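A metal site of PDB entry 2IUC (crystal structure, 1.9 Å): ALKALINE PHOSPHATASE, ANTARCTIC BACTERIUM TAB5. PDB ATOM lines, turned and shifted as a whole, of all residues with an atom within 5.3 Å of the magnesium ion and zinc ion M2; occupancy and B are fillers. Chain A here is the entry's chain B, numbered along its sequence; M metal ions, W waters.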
ATOM      1  N   ASP A  43      12.338 -27.470 -23.704  1.00  0.00           N
ATOM      2  CA  ASP A  43      12.487 -27.817 -25.103  1.00  0.00           C
ATOM      3  C   ASP A  43      12.523 -29.336 -25.268  1.00  0.00           C
ATOM      4  O   ASP A  43      13.296 -29.969 -24.609  1.00  0.00           O
ATOM      5  CB  ASP A  43      13.816 -27.226 -25.599  1.00  0.00           C
ATOM      6  CG  ASP A  43      13.909 -27.114 -27.157  1.00  0.00           C
ATOM      7  OD1 ASP A  43      13.826 -28.153 -27.840  1.00  0.00           O
ATOM      8  OD2 ASP A  43      14.183 -26.019 -27.669  1.00  0.00           O
ATOM      9  N   GLY A  44      11.723 -29.937 -26.158  1.00  0.00           N
ATOM     10  CA  GLY A  44      11.933 -31.371 -26.377  1.00  0.00           C
ATOM     11  C   GLY A  44      11.130 -32.209 -25.389  1.00  0.00           C
ATOM     12  O   GLY A  44      11.231 -33.413 -25.420  1.00  0.00           O
ATOM     13  N   ASP A  83      10.773 -27.879 -35.826  1.00  0.00           N
ATOM     14  CA  ASP A  83      12.034 -27.628 -35.039  1.00  0.00           C
ATOM     15  C   ASP A  83      11.806 -26.579 -33.946  1.00  0.00           C
ATOM     16  O   ASP A  83      10.703 -25.992 -33.840  1.00  0.00           O
ATOM     17  CB  ASP A  83      13.219 -27.328 -35.959  1.00  0.00           C
ATOM     18  CG  ASP A  83      13.300 -25.819 -36.429  1.00  0.00           C
ATOM     19  OD1 ASP A  83      12.285 -25.078 -36.504  1.00  0.00           O
ATOM     20  OD2 ASP A  83      14.424 -25.367 -36.736  1.00  0.00           O
ATOM     21  N   SER A  84      12.832 -26.291 -33.162  1.00  0.00           N
ATOM     22  CA  SER A  84      12.744 -25.292 -32.089  1.00  0.00           C
ATOM     23  C   SER A  84      12.472 -23.876 -32.556  1.00  0.00           C
ATOM     24  O   SER A  84      11.845 -23.086 -31.850  1.00  0.00           O
ATOM     25  CB  SER A  84      14.042 -25.279 -31.341  1.00  0.00           C
ATOM     26  OG  SER A  84      14.314 -26.617 -30.922  1.00  0.00           O
ATOM     27  N   SER A 131      21.088 -23.155 -22.780  1.00  0.00           N
ATOM     28  CA  SER A 131      21.893 -23.170 -24.001  1.00  0.00           C
ATOM     29  C   SER A 131      22.635 -21.833 -24.158  1.00  0.00           C
ATOM     30  O   SER A 131      22.549 -20.944 -23.285  1.00  0.00           O
ATOM     31  CB  SER A 131      20.953 -23.356 -25.235  1.00  0.00           C
ATOM     32  OG  SER A 131      20.015 -22.264 -25.329  1.00  0.00           O
ATOM     33  N   HIS A 135      20.766 -19.442 -29.219  1.00  0.00           N
ATOM     34  CA  HIS A 135      20.175 -20.727 -29.661  1.00  0.00           C
ATOM     35  C   HIS A 135      18.692 -20.532 -29.961  1.00  0.00           C
ATOM     36  O   HIS A 135      18.139 -19.501 -29.620  1.00  0.00           O
ATOM     37  CB  HIS A 135      20.459 -21.808 -28.638  1.00  0.00           C
ATOM     38  CG  HIS A 135      20.362 -23.188 -29.199  1.00  0.00           C
ATOM     39  ND1 HIS A 135      19.200 -23.922 -29.145  1.00  0.00           N
ATOM     40  CD2 HIS A 135      21.303 -24.005 -29.745  1.00  0.00           C
ATOM     41  CE1 HIS A 135      19.417 -25.116 -29.672  1.00  0.00           C
ATOM     42  NE2 HIS A 135      20.680 -25.188 -30.082  1.00  0.00           N
ATOM     43  N   ALA A 136      18.042 -21.437 -30.726  1.00  0.00           N
ATOM     44  CA  ALA A 136      16.822 -20.999 -31.453  1.00  0.00           C
ATOM     45  C   ALA A 136      15.665 -20.490 -30.576  1.00  0.00           C
ATOM     46  O   ALA A 136      14.880 -19.596 -30.973  1.00  0.00           O
ATOM     47  CB  ALA A 136      16.278 -22.144 -32.436  1.00  0.00           C
ATOM     48  N   THR A 137      15.473 -21.116 -29.393  1.00  0.00           N
ATOM     49  CA  THR A 137      14.332 -20.773 -28.512  1.00  0.00           C
ATOM     50  C   THR A 137      14.471 -19.357 -27.941  1.00  0.00           C
ATOM     51  O   THR A 137      13.587 -18.480 -28.245  1.00  0.00           O
ATOM     52  CB  THR A 137      14.130 -21.851 -27.406  1.00  0.00           C
ATOM     53  OG1 THR A 137      14.135 -23.145 -27.990  1.00  0.00           O
ATOM     54  CG2 THR A 137      12.805 -21.635 -26.566  1.00  0.00           C
ATOM     55  N   PRO A 138      15.597 -19.079 -27.197  1.00  0.00           N
ATOM     56  CA  PRO A 138      15.800 -17.673 -26.712  1.00  0.00           C
ATOM     57  C   PRO A 138      15.833 -16.659 -27.915  1.00  0.00           C
ATOM     58  O   PRO A 138      15.225 -15.600 -27.815  1.00  0.00           O
ATOM     59  CB  PRO A 138      17.111 -17.731 -25.928  1.00  0.00           C
ATOM     60  CG  PRO A 138      17.818 -19.061 -26.349  1.00  0.00           C
ATOM     61  CD  PRO A 138      16.722 -19.985 -26.824  1.00  0.00           C
ATOM     62  N   GLU A 254      14.031 -20.926 -20.401  1.00  0.00           N
ATOM     63  CA  GLU A 254      14.050 -22.160 -21.152  1.00  0.00           C
ATOM     64  C   GLU A 254      14.909 -23.197 -20.468  1.00  0.00           C
ATOM     65  O   GLU A 254      16.067 -22.906 -20.095  1.00  0.00           O
ATOM     66  CB  GLU A 254      14.599 -21.924 -22.542  1.00  0.00           C
ATOM     67  CG  GLU A 254      14.374 -23.157 -23.420  1.00  0.00           C
ATOM     68  CD  GLU A 254      15.291 -23.301 -24.628  1.00  0.00           C
ATOM     69  OE1 GLU A 254      16.318 -22.600 -24.701  1.00  0.00           O
ATOM     70  OE2 GLU A 254      15.026 -24.180 -25.510  1.00  0.00           O
ATOM     71  N   SER A 256      16.689 -25.726 -21.793  1.00  0.00           N
ATOM     72  CA  SER A 256      17.154 -25.930 -23.134  1.00  0.00           C
ATOM     73  C   SER A 256      17.670 -27.317 -23.447  1.00  0.00           C
ATOM     74  O   SER A 256      17.584 -27.777 -24.608  1.00  0.00           O
ATOM     75  CB  SER A 256      18.285 -24.922 -23.449  1.00  0.00           C
ATOM     76  OG  SER A 256      17.968 -23.608 -22.959  1.00  0.00           O
ATOM     77  N   ASP A 259      15.931 -31.332 -24.530  1.00  0.00           N
ATOM     78  CA  ASP A 259      16.028 -31.712 -25.949  1.00  0.00           C
ATOM     79  C   ASP A 259      17.293 -32.469 -26.328  1.00  0.00           C
ATOM     80  O   ASP A 259      17.291 -33.426 -27.096  1.00  0.00           O
ATOM     81  CB  ASP A 259      15.976 -30.431 -26.784  1.00  0.00           C
ATOM     82  CG  ASP A 259      16.006 -30.669 -28.306  1.00  0.00           C
ATOM     83  OD1 ASP A 259      15.099 -31.255 -28.843  1.00  0.00           O
ATOM     84  OD2 ASP A 259      16.924 -30.209 -28.986  1.00  0.00           O
ATOM     85  N   ASP A 301       8.066 -26.907 -26.945  1.00  0.00           N
ATOM     86  CA  ASP A 301       7.941 -26.576 -28.334  1.00  0.00           C
ATOM     87  C   ASP A 301       7.568 -27.828 -29.182  1.00  0.00           C
ATOM     88  O   ASP A 301       6.941 -27.687 -30.228  1.00  0.00           O
ATOM     89  CB  ASP A 301       9.236 -25.873 -28.843  1.00  0.00           C
ATOM     90  CG  ASP A 301      10.514 -26.688 -28.581  1.00  0.00           C
ATOM     91  OD1 ASP A 301      10.467 -27.623 -27.706  1.00  0.00           O
ATOM     92  OD2 ASP A 301      11.552 -26.399 -29.290  1.00  0.00           O
ATOM     93  N   HIS A 302       7.977 -28.996 -28.714  1.00  0.00           N
ATOM     94  CA  HIS A 302       7.791 -30.311 -29.411  1.00  0.00           C
ATOM     95  C   HIS A 302       8.393 -31.349 -28.433  1.00  0.00           C
ATOM     96  O   HIS A 302       9.028 -30.993 -27.385  1.00  0.00           O
ATOM     97  CB  HIS A 302       8.551 -30.357 -30.780  1.00  0.00           C
ATOM     98  CG  HIS A 302      10.031 -30.110 -30.616  1.00  0.00           C
ATOM     99  ND1 HIS A 302      10.915 -31.093 -30.162  1.00  0.00           N
ATOM    100  CD2 HIS A 302      10.757 -28.963 -30.704  1.00  0.00           C
ATOM    101  CE1 HIS A 302      12.116 -30.545 -29.987  1.00  0.00           C
ATOM    102  NE2 HIS A 302      12.046 -29.266 -30.338  1.00  0.00           N
ATOM    103  N   HIS A 337      12.885 -35.116 -33.511  1.00  0.00           N
ATOM    104  CA  HIS A 337      11.691 -34.627 -32.869  1.00  0.00           C
ATOM    105  C   HIS A 337      10.491 -35.512 -33.269  1.00  0.00           C
ATOM    106  O   HIS A 337      10.558 -36.273 -34.248  1.00  0.00           O
ATOM    107  CB  HIS A 337      11.381 -33.147 -33.267  1.00  0.00           C
ATOM    108  CG  HIS A 337      12.491 -32.192 -32.929  1.00  0.00           C
ATOM    109  ND1 HIS A 337      12.513 -30.895 -33.396  1.00  0.00           N
ATOM    110  CD2 HIS A 337      13.636 -32.374 -32.232  1.00  0.00           C
ATOM    111  CE1 HIS A 337      13.633 -30.300 -32.974  1.00  0.00           C
ATOM    112  NE2 HIS A 337      14.304 -31.177 -32.249  1.00  0.00           N
HETATM  113 MG    MG M   1      15.750 -24.543 -27.224  1.00  0.00          MG
HETATM  114 ZN    ZN M   2      13.120 -27.730 -29.604  1.00  0.00          ZN
HETATM  115 ZN    ZN M   3      15.943 -30.835 -31.014  1.00  0.00          ZN
HETATM  116  O   HOH W   1      17.059 -26.194 -26.794  1.00  0.00           O
HETATM  117  O   HOH W   2      16.361 -24.710 -29.479  1.00  0.00           O
HETATM  118  O   HOH W   3      17.435 -23.159 -27.279  1.00  0.00           O
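Four residues have an atom within 4 Å of zinc ion M2: Asp 43, Ser 84, Asp 301 and His 302.
His 135 touches the magnesium ion (ND1 to MG, 3.997 Å). Within 4 Å of the magnesium ion: Asp 43, His 135, Thr 137 and Glu 254. The nearest printed residue that does not touch the magnesium ion is Ser 84 (4.5 Å).
Zinc ion M2 is bound by OD1 of Asp 43 (1.9 Å), NE2 of His 302 (2.0 Å), OD2 of Asp 301 (2.1 Å) and OG of Ser 84 (2.1 Å). Slightly farther from zinc ion M2 lies OD2 of Asp 43 (2.8 Å).
Water W3 lies within hydrogen-bond range of ND1 of His 135 (2.7 Å), OE1 of Glu 254 (2.9 Å) and OG of Ser 131 (3.4 Å).
O of His 302 lies close to N of Gly 44, 3.1 Å away. The side-chain carboxylate (OD1) of Asp 301 sits at hydrogen-bond distance from the backbone NH (N) of Gly 44 (3.1 Å). The side-chain carboxylate of Glu 254 lies within hydrogen-bond range of the side-chain hydroxyl of Ser 256, at 2.6 Å. NE2 of His 302 lies close to ND1 of His 337 (3.5 Å). N of Asp 259 lies within hydrogen-bond range of O of Asp 43 (3.0 Å).
The magnesium ion is bound by OE2 of Glu 254 (1.9 Å), water W1 (2.2 Å), water W3 (2.2 Å), OD2 of Asp 43 (2.2 Å), OG1 of Thr 137 (2.3 Å) and water W2 (2.3 Å).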
